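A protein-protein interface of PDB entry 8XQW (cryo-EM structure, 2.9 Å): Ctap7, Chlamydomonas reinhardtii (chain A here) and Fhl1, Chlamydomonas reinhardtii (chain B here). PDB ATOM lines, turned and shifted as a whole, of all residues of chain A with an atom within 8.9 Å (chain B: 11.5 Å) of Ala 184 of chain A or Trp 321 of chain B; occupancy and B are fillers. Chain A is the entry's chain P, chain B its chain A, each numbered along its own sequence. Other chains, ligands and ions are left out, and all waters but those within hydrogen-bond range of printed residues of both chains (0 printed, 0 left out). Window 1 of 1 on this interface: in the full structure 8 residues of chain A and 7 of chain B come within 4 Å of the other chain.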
ATOM      1  N   ASP A  57     -35.729 -32.009 -31.900  1.00  0.00           N
ATOM      2  CA  ASP A  57     -35.710 -30.596 -31.547  1.00  0.00           C
ATOM      3  C   ASP A  57     -37.060 -29.952 -31.857  1.00  0.00           C
ATOM      4  O   ASP A  57     -37.784 -30.404 -32.741  1.00  0.00           O
ATOM      5  CB  ASP A  57     -34.579 -29.880 -32.287  1.00  0.00           C
ATOM      6  CG  ASP A  57     -34.743 -28.377 -32.295  1.00  0.00           C
ATOM      7  OD1 ASP A  57     -34.566 -27.755 -31.226  1.00  0.00           O
ATOM      8  OD2 ASP A  57     -35.057 -27.821 -33.366  1.00  0.00           O
ATOM      9  N   LEU A  58     -37.395 -28.899 -31.115  1.00  0.00           N
ATOM     10  CA  LEU A  58     -38.680 -28.223 -31.248  1.00  0.00           C
ATOM     11  C   LEU A  58     -38.687 -27.268 -32.434  1.00  0.00           C
ATOM     12  O   LEU A  58     -37.846 -27.378 -33.333  1.00  0.00           O
ATOM     13  CB  LEU A  58     -39.031 -27.480 -29.959  1.00  0.00           C
ATOM     14  CG  LEU A  58     -40.501 -27.544 -29.528  1.00  0.00           C
ATOM     15  CD1 LEU A  58     -41.142 -28.837 -29.986  1.00  0.00           C
ATOM     16  CD2 LEU A  58     -40.640 -27.402 -28.024  1.00  0.00           C
ATOM     17  N   ARG A  60     -41.372 -26.717 -34.805  1.00  0.00           N
ATOM     18  CA  ARG A  60     -41.992 -27.256 -36.009  1.00  0.00           C
ATOM     19  C   ARG A  60     -43.315 -26.535 -36.238  1.00  0.00           C
ATOM     20  O   ARG A  60     -44.388 -27.104 -36.003  1.00  0.00           O
ATOM     21  CB  ARG A  60     -42.189 -28.766 -35.888  1.00  0.00           C
ATOM     22  CG  ARG A  60     -40.918 -29.503 -35.504  1.00  0.00           C
ATOM     23  CD  ARG A  60     -39.794 -29.147 -36.458  1.00  0.00           C
ATOM     24  NE  ARG A  60     -38.594 -28.687 -35.764  1.00  0.00           N
ATOM     25  CZ  ARG A  60     -37.521 -29.440 -35.546  1.00  0.00           C
ATOM     26  NH1 ARG A  60     -37.497 -30.701 -35.954  1.00  0.00           N
ATOM     27  NH2 ARG A  60     -36.472 -28.935 -34.911  1.00  0.00           N
ATOM     28  N   LEU A 173     -34.051 -38.920 -26.409  1.00  0.00           N
ATOM     29  CA  LEU A 173     -34.217 -37.769 -25.534  1.00  0.00           C
ATOM     30  C   LEU A 173     -34.848 -38.176 -24.214  1.00  0.00           C
ATOM     31  O   LEU A 173     -34.551 -37.581 -23.173  1.00  0.00           O
ATOM     32  CB  LEU A 173     -35.052 -36.703 -26.227  1.00  0.00           C
ATOM     33  CG  LEU A 173     -34.231 -35.644 -26.952  1.00  0.00           C
ATOM     34  CD1 LEU A 173     -35.066 -34.974 -28.020  1.00  0.00           C
ATOM     35  CD2 LEU A 173     -33.704 -34.626 -25.958  1.00  0.00           C
ATOM     36  N   LEU A 176     -31.952 -39.385 -22.276  1.00  0.00           N
ATOM     37  CA  LEU A 176     -31.117 -38.261 -21.871  1.00  0.00           C
ATOM     38  C   LEU A 176     -31.715 -37.551 -20.668  1.00  0.00           C
ATOM     39  O   LEU A 176     -31.006 -37.199 -19.720  1.00  0.00           O
ATOM     40  CB  LEU A 176     -30.938 -37.293 -23.036  1.00  0.00           C
ATOM     41  CG  LEU A 176     -29.497 -37.132 -23.504  1.00  0.00           C
ATOM     42  CD1 LEU A 176     -29.426 -36.176 -24.671  1.00  0.00           C
ATOM     43  CD2 LEU A 176     -28.643 -36.643 -22.357  1.00  0.00           C
ATOM     44  N   ARG A 181     -27.155 -35.537 -16.867  1.00  0.00           N
ATOM     45  CA  ARG A 181     -25.888 -35.014 -17.368  1.00  0.00           C
ATOM     46  C   ARG A 181     -26.043 -33.620 -17.948  1.00  0.00           C
ATOM     47  O   ARG A 181     -26.863 -33.391 -18.841  1.00  0.00           O
ATOM     48  CB  ARG A 181     -25.326 -35.961 -18.424  1.00  0.00           C
ATOM     49  CG  ARG A 181     -24.081 -35.424 -19.083  1.00  0.00           C
ATOM     50  CD  ARG A 181     -23.691 -36.246 -20.279  1.00  0.00           C
ATOM     51  NE  ARG A 181     -23.785 -37.669 -20.004  1.00  0.00           N
ATOM     52  CZ  ARG A 181     -22.902 -38.559 -20.432  1.00  0.00           C
ATOM     53  NH1 ARG A 181     -21.861 -38.161 -21.147  1.00  0.00           N
ATOM     54  NH2 ARG A 181     -23.053 -39.844 -20.139  1.00  0.00           N
ATOM     55  N   ARG A 182     -25.263 -32.686 -17.421  1.00  0.00           N
ATOM     56  CA  ARG A 182     -25.359 -31.286 -17.804  1.00  0.00           C
ATOM     57  C   ARG A 182     -24.332 -30.992 -18.888  1.00  0.00           C
ATOM     58  O   ARG A 182     -23.131 -30.922 -18.612  1.00  0.00           O
ATOM     59  CB  ARG A 182     -25.145 -30.384 -16.592  1.00  0.00           C
ATOM     60  CG  ARG A 182     -25.972 -29.114 -16.633  1.00  0.00           C
ATOM     61  CD  ARG A 182     -26.258 -28.581 -15.241  1.00  0.00           C
ATOM     62  NE  ARG A 182     -25.111 -28.720 -14.351  1.00  0.00           N
ATOM     63  CZ  ARG A 182     -25.093 -29.501 -13.276  1.00  0.00           C
ATOM     64  NH1 ARG A 182     -26.162 -30.216 -12.955  1.00  0.00           N
ATOM     65  NH2 ARG A 182     -24.006 -29.568 -12.525  1.00  0.00           N
ATOM     66  N   ILE A 183     -24.808 -30.814 -20.115  1.00  0.00           N
ATOM     67  CA  ILE A 183     -23.960 -30.594 -21.278  1.00  0.00           C
ATOM     68  C   ILE A 183     -23.959 -29.108 -21.588  1.00  0.00           C
ATOM     69  O   ILE A 183     -24.994 -28.545 -21.959  1.00  0.00           O
ATOM     70  CB  ILE A 183     -24.449 -31.405 -22.485  1.00  0.00           C
ATOM     71  CG1 ILE A 183     -24.432 -32.891 -22.155  1.00  0.00           C
ATOM     72  CG2 ILE A 183     -23.592 -31.132 -23.692  1.00  0.00           C
ATOM     73  CD1 ILE A 183     -25.115 -33.731 -23.188  1.00  0.00           C
ATOM     74  N   ALA A 184     -22.802 -28.471 -21.435  1.00  0.00           N
ATOM     75  CA  ALA A 184     -22.680 -27.060 -21.752  1.00  0.00           C
ATOM     76  C   ALA A 184     -23.005 -26.818 -23.218  1.00  0.00           C
ATOM     77  O   ALA A 184     -22.977 -27.728 -24.047  1.00  0.00           O
ATOM     78  CB  ALA A 184     -21.275 -26.557 -21.438  1.00  0.00           C
ATOM     79  N   VAL A 185     -23.325 -25.569 -23.536  1.00  0.00           N
ATOM     80  CA  VAL A 185     -23.718 -25.176 -24.881  1.00  0.00           C
ATOM     81  C   VAL A 185     -22.703 -24.172 -25.404  1.00  0.00           C
ATOM     82  O   VAL A 185     -22.184 -23.349 -24.642  1.00  0.00           O
ATOM     83  CB  VAL A 185     -25.148 -24.609 -24.909  1.00  0.00           C
ATOM     84  CG1 VAL A 185     -25.215 -23.276 -24.212  1.00  0.00           C
ATOM     85  CG2 VAL A 185     -25.644 -24.487 -26.331  1.00  0.00           C
ATOM     86  N   ALA A 186     -22.397 -24.263 -26.695  1.00  0.00           N
ATOM     87  CA  ALA A 186     -21.384 -23.413 -27.299  1.00  0.00           C
ATOM     88  C   ALA A 186     -22.002 -22.138 -27.851  1.00  0.00           C
ATOM     89  O   ALA A 186     -23.102 -22.151 -28.407  1.00  0.00           O
ATOM     90  CB  ALA A 186     -20.657 -24.161 -28.412  1.00  0.00           C
ATOM     91  N   ASP A 187     -21.285 -21.036 -27.689  1.00  0.00           N
ATOM     92  CA  ASP A 187     -21.748 -19.734 -28.141  1.00  0.00           C
ATOM     93  C   ASP A 187     -21.881 -19.733 -29.659  1.00  0.00           C
ATOM     94  O   ASP A 187     -20.880 -19.942 -30.357  1.00  0.00           O
ATOM     95  CB  ASP A 187     -20.772 -18.657 -27.692  1.00  0.00           C
ATOM     96  CG  ASP A 187     -21.328 -17.264 -27.856  1.00  0.00           C
ATOM     97  OD1 ASP A 187     -22.169 -17.049 -28.748  1.00  0.00           O
ATOM     98  OD2 ASP A 187     -20.937 -16.377 -27.071  1.00  0.00           O
ATOM     99  N   PRO A 188     -23.070 -19.484 -30.209  1.00  0.00           N
ATOM    100  CA  PRO A 188     -23.250 -19.604 -31.663  1.00  0.00           C
ATOM    101  C   PRO A 188     -22.504 -18.563 -32.483  1.00  0.00           C
ATOM    102  O   PRO A 188     -22.583 -18.621 -33.715  1.00  0.00           O
ATOM    103  CB  PRO A 188     -24.765 -19.464 -31.846  1.00  0.00           C
ATOM    104  CG  PRO A 188     -25.348 -19.697 -30.496  1.00  0.00           C
ATOM    105  CD  PRO A 188     -24.338 -19.202 -29.523  1.00  0.00           C
ATOM    106  N   GLY A 193     -16.375 -20.544 -29.962  1.00  0.00           N
ATOM    107  CA  GLY A 193     -17.406 -21.431 -29.467  1.00  0.00           C
ATOM    108  C   GLY A 193     -17.205 -21.869 -28.037  1.00  0.00           C
ATOM    109  O   GLY A 193     -17.688 -22.937 -27.651  1.00  0.00           O
ATOM    110  N   ARG A 194     -16.487 -21.079 -27.245  1.00  0.00           N
ATOM    111  CA  ARG A 194     -16.291 -21.402 -25.844  1.00  0.00           C
ATOM    112  C   ARG A 194     -17.641 -21.481 -25.135  1.00  0.00           C
ATOM    113  O   ARG A 194     -18.595 -20.805 -25.524  1.00  0.00           O
ATOM    114  CB  ARG A 194     -15.407 -20.352 -25.180  1.00  0.00           C
ATOM    115  CG  ARG A 194     -14.048 -20.216 -25.825  1.00  0.00           C
ATOM    116  CD  ARG A 194     -13.427 -18.882 -25.494  1.00  0.00           C
ATOM    117  NE  ARG A 194     -14.100 -17.788 -26.186  1.00  0.00           N
ATOM    118  CZ  ARG A 194     -13.477 -16.888 -26.938  1.00  0.00           C
ATOM    119  NH1 ARG A 194     -14.168 -15.928 -27.532  1.00  0.00           N
ATOM    120  NH2 ARG A 194     -12.163 -16.949 -27.097  1.00  0.00           N
ATOM    121  N   PRO A 195     -17.750 -22.308 -24.100  1.00  0.00           N
ATOM    122  CA  PRO A 195     -19.040 -22.471 -23.425  1.00  0.00           C
ATOM    123  C   PRO A 195     -19.543 -21.158 -22.853  1.00  0.00           C
ATOM    124  O   PRO A 195     -18.768 -20.286 -22.453  1.00  0.00           O
ATOM    125  CB  PRO A 195     -18.737 -23.486 -22.319  1.00  0.00           C
ATOM    126  CG  PRO A 195     -17.268 -23.447 -22.154  1.00  0.00           C
ATOM    127  CD  PRO A 195     -16.714 -23.164 -23.506  1.00  0.00           C
ATOM    128  N   LEU A 196     -20.863 -21.022 -22.829  1.00  0.00           N
ATOM    129  CA  LEU A 196     -21.480 -19.786 -22.388  1.00  0.00           C
ATOM    130  C   LEU A 196     -21.394 -19.658 -20.869  1.00  0.00           C
ATOM    131  O   LEU A 196     -21.286 -20.658 -20.158  1.00  0.00           O
ATOM    132  CB  LEU A 196     -22.937 -19.737 -22.834  1.00  0.00           C
ATOM    133  CG  LEU A 196     -23.134 -19.517 -24.331  1.00  0.00           C
ATOM    134  CD1 LEU A 196     -24.567 -19.795 -24.731  1.00  0.00           C
ATOM    135  CD2 LEU A 196     -22.740 -18.105 -24.698  1.00  0.00           C
ATOM    136  N   PRO A 197     -21.443 -18.430 -20.347  1.00  0.00           N
ATOM    137  CA  PRO A 197     -21.377 -18.224 -18.897  1.00  0.00           C
ATOM    138  C   PRO A 197     -22.659 -18.555 -18.152  1.00  0.00           C
ATOM    139  O   PRO A 197     -22.797 -18.148 -16.994  1.00  0.00           O
ATOM    140  CB  PRO A 197     -21.058 -16.722 -18.774  1.00  0.00           C
ATOM    141  CG  PRO A 197     -20.671 -16.268 -20.145  1.00  0.00           C
ATOM    142  CD  PRO A 197     -21.406 -17.157 -21.081  1.00  0.00           C
ATOM    143  N   GLY A 198     -23.598 -19.257 -18.779  1.00  0.00           N
ATOM    144  CA  GLY A 198     -24.826 -19.645 -18.115  1.00  0.00           C
ATOM    145  C   GLY A 198     -24.599 -20.441 -16.849  1.00  0.00           C
ATOM    146  O   GLY A 198     -24.911 -19.969 -15.752  1.00  0.00           O
ATOM    147  N   GLY A 199     -24.052 -21.645 -16.983  1.00  0.00           N
ATOM    148  CA  GLY A 199     -23.805 -22.468 -15.810  1.00  0.00           C
ATOM    149  C   GLY A 199     -25.101 -22.817 -15.107  1.00  0.00           C
ATOM    150  O   GLY A 199     -26.019 -23.398 -15.694  1.00  0.00           O
ATOM    151  N   ARG B 315     -10.227 -31.501 -16.129  1.00  0.00           N
ATOM    152  CA  ARG B 315     -11.572 -32.057 -16.058  1.00  0.00           C
ATOM    153  C   ARG B 315     -12.645 -31.062 -16.455  1.00  0.00           C
ATOM    154  O   ARG B 315     -13.829 -31.397 -16.404  1.00  0.00           O
ATOM    155  CB  ARG B 315     -11.865 -32.574 -14.654  1.00  0.00           C
ATOM    156  CG  ARG B 315     -12.316 -31.502 -13.691  1.00  0.00           C
ATOM    157  CD  ARG B 315     -12.236 -31.998 -12.275  1.00  0.00           C
ATOM    158  NE  ARG B 315     -12.262 -30.913 -11.310  1.00  0.00           N
ATOM    159  CZ  ARG B 315     -11.874 -31.043 -10.049  1.00  0.00           C
ATOM    160  NH1 ARG B 315     -11.436 -32.210  -9.616  1.00  0.00           N
ATOM    161  NH2 ARG B 315     -11.921 -30.012  -9.227  1.00  0.00           N
ATOM    162  N   ALA B 316     -12.266 -29.856 -16.850  1.00  0.00           N
ATOM    163  CA  ALA B 316     -13.228 -28.817 -17.179  1.00  0.00           C
ATOM    164  C   ALA B 316     -13.577 -28.772 -18.656  1.00  0.00           C
ATOM    165  O   ALA B 316     -14.040 -27.732 -19.134  1.00  0.00           O
ATOM    166  CB  ALA B 316     -12.699 -27.451 -16.742  1.00  0.00           C
ATOM    167  N   GLU B 317     -13.361 -29.854 -19.393  1.00  0.00           N
ATOM    168  CA  GLU B 317     -13.651 -29.895 -20.817  1.00  0.00           C
ATOM    169  C   GLU B 317     -14.426 -31.160 -21.149  1.00  0.00           C
ATOM    170  O   GLU B 317     -14.163 -32.225 -20.588  1.00  0.00           O
ATOM    171  CB  GLU B 317     -12.367 -29.836 -21.644  1.00  0.00           C
ATOM    172  CG  GLU B 317     -11.494 -28.627 -21.356  1.00  0.00           C
ATOM    173  CD  GLU B 317     -11.887 -27.409 -22.169  1.00  0.00           C
ATOM    174  OE1 GLU B 317     -11.066 -26.475 -22.278  1.00  0.00           O
ATOM    175  OE2 GLU B 317     -13.018 -27.376 -22.699  1.00  0.00           O
ATOM    176  N   GLY B 318     -15.375 -31.035 -22.061  1.00  0.00           N
ATOM    177  CA  GLY B 318     -16.158 -32.180 -22.460  1.00  0.00           C
ATOM    178  C   GLY B 318     -16.935 -31.898 -23.723  1.00  0.00           C
ATOM    179  O   GLY B 318     -16.670 -30.926 -24.428  1.00  0.00           O
ATOM    180  N   ALA B 319     -17.898 -32.767 -24.003  1.00  0.00           N
ATOM    181  CA  ALA B 319     -18.743 -32.575 -25.167  1.00  0.00           C
ATOM    182  C   ALA B 319     -19.696 -31.414 -24.937  1.00  0.00           C
ATOM    183  O   ALA B 319     -20.142 -31.155 -23.818  1.00  0.00           O
ATOM    184  CB  ALA B 319     -19.528 -33.845 -25.475  1.00  0.00           C
ATOM    185  N   VAL B 320     -20.008 -30.700 -26.016  1.00  0.00           N
ATOM    186  CA  VAL B 320     -20.915 -29.565 -25.943  1.00  0.00           C
ATOM    187  C   VAL B 320     -21.923 -29.670 -27.073  1.00  0.00           C
ATOM    188  O   VAL B 320     -21.765 -30.468 -28.001  1.00  0.00           O
ATOM    189  CB  VAL B 320     -20.174 -28.216 -26.018  1.00  0.00           C
ATOM    190  CG1 VAL B 320     -19.344 -27.999 -24.776  1.00  0.00           C
ATOM    191  CG2 VAL B 320     -19.312 -28.170 -27.248  1.00  0.00           C
ATOM    192  N   TRP B 321     -22.973 -28.867 -26.982  1.00  0.00           N
ATOM    193  CA  TRP B 321     -23.980 -28.774 -28.023  1.00  0.00           C
ATOM    194  C   TRP B 321     -23.775 -27.466 -28.771  1.00  0.00           C
ATOM    195  O   TRP B 321     -23.739 -26.399 -28.153  1.00  0.00           O
ATOM    196  CB  TRP B 321     -25.388 -28.836 -27.435  1.00  0.00           C
ATOM    197  CG  TRP B 321     -26.422 -28.305 -28.364  1.00  0.00           C
ATOM    198  CD1 TRP B 321     -26.907 -27.035 -28.412  1.00  0.00           C
ATOM    199  CD2 TRP B 321     -27.095 -29.032 -29.392  1.00  0.00           C
ATOM    200  NE1 TRP B 321     -27.839 -26.924 -29.409  1.00  0.00           N
ATOM    201  CE2 TRP B 321     -27.972 -28.140 -30.025  1.00  0.00           C
ATOM    202  CE3 TRP B 321     -27.039 -30.352 -29.840  1.00  0.00           C
ATOM    203  CZ2 TRP B 321     -28.786 -28.522 -31.080  1.00  0.00           C
ATOM    204  CZ3 TRP B 321     -27.849 -30.730 -30.885  1.00  0.00           C
ATOM    205  CH2 TRP B 321     -28.712 -29.821 -31.492  1.00  0.00           C
ATOM    206  N   ASP B 322     -23.635 -27.545 -30.088  1.00  0.00           N
ATOM    207  CA  ASP B 322     -23.561 -26.332 -30.882  1.00  0.00           C
ATOM    208  C   ASP B 322     -24.876 -26.139 -31.612  1.00  0.00           C
ATOM    209  O   ASP B 322     -25.253 -26.995 -32.430  1.00  0.00           O
ATOM    210  CB  ASP B 322     -22.412 -26.385 -31.875  1.00  0.00           C
ATOM    211  CG  ASP B 322     -22.396 -25.185 -32.788  1.00  0.00           C
ATOM    212  OD1 ASP B 322     -22.124 -24.073 -32.295  1.00  0.00           O
ATOM    213  OD2 ASP B 322     -22.671 -25.344 -33.992  1.00  0.00           O
ATOM    214  N   PRO B 323     -25.604 -25.060 -31.350  1.00  0.00           N
ATOM    215  CA  PRO B 323     -26.878 -24.837 -32.039  1.00  0.00           C
ATOM    216  C   PRO B 323     -26.686 -24.207 -33.405  1.00  0.00           C
ATOM    217  O   PRO B 323     -27.584 -24.253 -34.250  1.00  0.00           O
ATOM    218  CB  PRO B 323     -27.617 -23.899 -31.086  1.00  0.00           C
ATOM    219  CG  PRO B 323     -26.526 -23.121 -30.439  1.00  0.00           C
ATOM    220  CD  PRO B 323     -25.349 -24.045 -30.316  1.00  0.00           C
ATOM    221  N   ALA B 324     -25.518 -23.601 -33.628  1.00  0.00           N
ATOM    222  CA  ALA B 324     -25.229 -23.038 -34.942  1.00  0.00           C
ATOM    223  C   ALA B 324     -25.129 -24.126 -35.996  1.00  0.00           C
ATOM    224  O   ALA B 324     -25.417 -23.882 -37.171  1.00  0.00           O
ATOM    225  CB  ALA B 324     -23.938 -22.224 -34.895  1.00  0.00           C
ATOM    226  N   SER B 325     -24.720 -25.325 -35.601  1.00  0.00           N
ATOM    227  CA  SER B 325     -24.764 -26.480 -36.475  1.00  0.00           C
ATOM    228  C   SER B 325     -25.731 -27.548 -35.998  1.00  0.00           C
ATOM    229  O   SER B 325     -25.925 -28.541 -36.705  1.00  0.00           O
ATOM    230  CB  SER B 325     -23.368 -27.104 -36.618  1.00  0.00           C
ATOM    231  OG  SER B 325     -23.240 -28.228 -35.773  1.00  0.00           O
ATOM    232  N   GLY B 326     -26.342 -27.373 -34.832  1.00  0.00           N
ATOM    233  CA  GLY B 326     -27.271 -28.346 -34.306  1.00  0.00           C
ATOM    234  C   GLY B 326     -26.637 -29.705 -34.125  1.00  0.00           C
ATOM    235  O   GLY B 326     -27.200 -30.717 -34.549  1.00  0.00           O
ATOM    236  N   GLN B 327     -25.468 -29.748 -33.494  1.00  0.00           N
ATOM    237  CA  GLN B 327     -24.741 -31.003 -33.386  1.00  0.00           C
ATOM    238  C   GLN B 327     -24.121 -31.125 -32.005  1.00  0.00           C
ATOM    239  O   GLN B 327     -24.108 -30.181 -31.215  1.00  0.00           O
ATOM    240  CB  GLN B 327     -23.659 -31.110 -34.457  1.00  0.00           C
ATOM    241  CG  GLN B 327     -24.179 -31.429 -35.836  1.00  0.00           C
ATOM    242  CD  GLN B 327     -23.332 -32.458 -36.541  1.00  0.00           C
ATOM    243  OE1 GLN B 327     -23.721 -33.615 -36.670  1.00  0.00           O
ATOM    244  NE2 GLN B 327     -22.160 -32.042 -36.996  1.00  0.00           N
ATOM    245  N   TYR B 328     -23.613 -32.318 -31.723  1.00  0.00           N
ATOM    246  CA  TYR B 328     -22.820 -32.569 -30.533  1.00  0.00           C
ATOM    247  C   TYR B 328     -21.353 -32.575 -30.924  1.00  0.00           C
ATOM    248  O   TYR B 328     -20.914 -33.427 -31.700  1.00  0.00           O
ATOM    249  CB  TYR B 328     -23.205 -33.894 -29.883  1.00  0.00           C
ATOM    250  CG  TYR B 328     -24.521 -33.834 -29.162  1.00  0.00           C
ATOM    251  CD1 TYR B 328     -24.704 -32.977 -28.095  1.00  0.00           C
ATOM    252  CD2 TYR B 328     -25.579 -34.627 -29.550  1.00  0.00           C
ATOM    253  CE1 TYR B 328     -25.902 -32.913 -27.434  1.00  0.00           C
ATOM    254  CE2 TYR B 328     -26.781 -34.570 -28.893  1.00  0.00           C
ATOM    255  CZ  TYR B 328     -26.939 -33.711 -27.837  1.00  0.00           C
ATOM    256  OH  TYR B 328     -28.140 -33.655 -27.180  1.00  0.00           O
ATOM    257  N   ILE B 329     -20.603 -31.624 -30.385  1.00  0.00           N
ATOM    258  CA  ILE B 329     -19.226 -31.382 -30.784  1.00  0.00           C
ATOM    259  C   ILE B 329     -18.315 -31.757 -29.629  1.00  0.00           C
ATOM    260  O   ILE B 329     -18.565 -31.364 -28.483  1.00  0.00           O
ATOM    261  CB  ILE B 329     -19.014 -29.910 -31.178  1.00  0.00           C
ATOM    262  CG1 ILE B 329     -19.870 -29.550 -32.388  1.00  0.00           C
ATOM    263  CG2 ILE B 329     -17.560 -29.642 -31.460  1.00  0.00           C
ATOM    264  CD1 ILE B 329     -19.252 -29.926 -33.701  1.00  0.00           C
ATOM    265  N   LEU B 330     -17.264 -32.517 -29.925  1.00  0.00           N
ATOM    266  CA  LEU B 330     -16.169 -32.681 -28.982  1.00  0.00           C
ATOM    267  C   LEU B 330     -15.080 -31.696 -29.370  1.00  0.00           C
ATOM    268  O   LEU B 330     -14.312 -31.970 -30.300  1.00  0.00           O
ATOM    269  CB  LEU B 330     -15.631 -34.108 -28.991  1.00  0.00           C
ATOM    270  CG  LEU B 330     -14.531 -34.303 -27.957  1.00  0.00           C
ATOM    271  CD1 LEU B 330     -15.047 -33.940 -26.592  1.00  0.00           C
ATOM    272  CD2 LEU B 330     -14.037 -35.725 -27.965  1.00  0.00           C
ATOM    273  N   PRO B 331     -14.975 -30.549 -28.707  1.00  0.00           N
ATOM    274  CA  PRO B 331     -14.094 -29.488 -29.197  1.00  0.00           C
ATOM    275  C   PRO B 331     -12.642 -29.927 -29.255  1.00  0.00           C
ATOM    276  O   PRO B 331     -12.215 -30.855 -28.570  1.00  0.00           O
ATOM    277  CB  PRO B 331     -14.296 -28.366 -28.177  1.00  0.00           C
ATOM    278  CG  PRO B 331     -14.809 -29.041 -26.974  1.00  0.00           C
ATOM    279  CD  PRO B 331     -15.636 -30.176 -27.453  1.00  0.00           C
ATOM    280  N   ARG B 333      -9.956 -28.356 -28.296  1.00  0.00           N
ATOM    281  CA  ARG B 333      -9.131 -28.101 -27.124  1.00  0.00           C
ATOM    282  C   ARG B 333      -9.400 -29.054 -26.006  1.00  0.00           C
ATOM    283  O   ARG B 333      -8.891 -28.858 -24.903  1.00  0.00           O
ATOM    284  CB  ARG B 333      -9.321 -26.663 -26.651  1.00  0.00           C
ATOM    285  CG  ARG B 333     -10.565 -26.427 -25.843  1.00  0.00           C
ATOM    286  CD  ARG B 333     -10.802 -24.942 -25.649  1.00  0.00           C
ATOM    287  NE  ARG B 333     -11.591 -24.384 -26.741  1.00  0.00           N
ATOM    288  CZ  ARG B 333     -12.913 -24.461 -26.815  1.00  0.00           C
ATOM    289  NH1 ARG B 333     -13.597 -25.072 -25.859  1.00  0.00           N
ATOM    290  NH2 ARG B 333     -13.552 -23.928 -27.846  1.00  0.00           N
ATOM    291  N   ALA B 334     -10.184 -30.100 -26.253  1.00  0.00           N
ATOM    292  CA  ALA B 334     -10.410 -31.158 -25.283  1.00  0.00           C
ATOM    293  C   ALA B 334      -9.895 -32.502 -25.768  1.00  0.00           C
ATOM    294  O   ALA B 334     -10.185 -33.525 -25.140  1.00  0.00           O
ATOM    295  CB  ALA B 334     -11.896 -31.264 -24.945  1.00  0.00           C
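The backbone carbonyl oxygen (O) of Ala 184 of chain A is in hydrogen-bond range of the backbone NH (N) of Trp 321 of chain B, at 3.1 Å.
The backbone carbonyl oxygen (O) of Trp 321 of chain B lies within hydrogen-bond range of the backbone NH (N) of Ala 186 of chain A, at 2.9 Å.
The backbone carbonyl oxygen (O) of Val 320 of chain B lies within hydrogen-bond range of the backbone NH (N) of Ile 329 of chain B (2.9 Å).
O of Val 185 of chain A lies within hydrogen-bond range of N of Leu 196 of chain A (3.2 Å).
Among the printed residues, merely in contact across the chains: Leu 176 of chain A with Tyr 328 of chain B (3.8 Å), Ile 183 of chain A with Ala 319 of chain B (3.5 Å), Ile 183 of chain A with Val 320 of chain B (3.8 Å), Ala 184 of chain A with Val 320 of chain B (3.3 Å), Val 185 of chain A with Trp 321 of chain B (3.3 Å), Ala 186 of chain A with Pro 323 of chain B (3.5 Å) and Pro 188 of chain A with Pro 323 of chain B (3.6 Å).
Ala 184 of chain A touches just these residues of chain B: Val 320 (3.3 Å) and Trp 321 (3.1 Å).
Of chain A, only Ala 184, Val 185 and Ala 186 come within 4 Å of Trp 321 of chain B.
Val 185 of chain A touches just one residue of chain B: Trp 321 (3.3 Å).
Ala 186 of chain A touches two residues of chain B.
Pro 195 of chain A touches none of the printed residues of chain B.
No residue of chain A comes within 4 Å of Gly 326 of chain B.
Of the printed residues of chain A, Pro 323 of chain B touches Ala 186 and Pro 188.
Of the printed residues of chain B, Pro 188 of chain A touches Pro 323 (3.6 Å).
Of the printed residues of chain A, Tyr 328 of chain B touches Leu 176.
Printed residues of chain A within 4 Å of Ala 319 of chain B: Ile 183 (3.5 Å).
Printed residues of chain B within 4 Å of Leu 176 of chain A: Tyr 328.
The nearest residue of chain A that does not touch Trp 321 of chain B is Ile 183 of chain A (4.04 Å).
Hydrophobic or aromatic side chains of chain A that line the printed part of chain B: Leu 176, Ile 183, Val 185, Ala 186 and Pro 188.
Of the 19 printed residues of chain B, 5 touch a printed residue of chain A.
Among the printed residues, 9 pairs touch across the chains.
Among the printed residues, no Asp or Glu carboxylate lies within 4 Å of a Lys or Arg side-chain nitrogen of the other chain.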
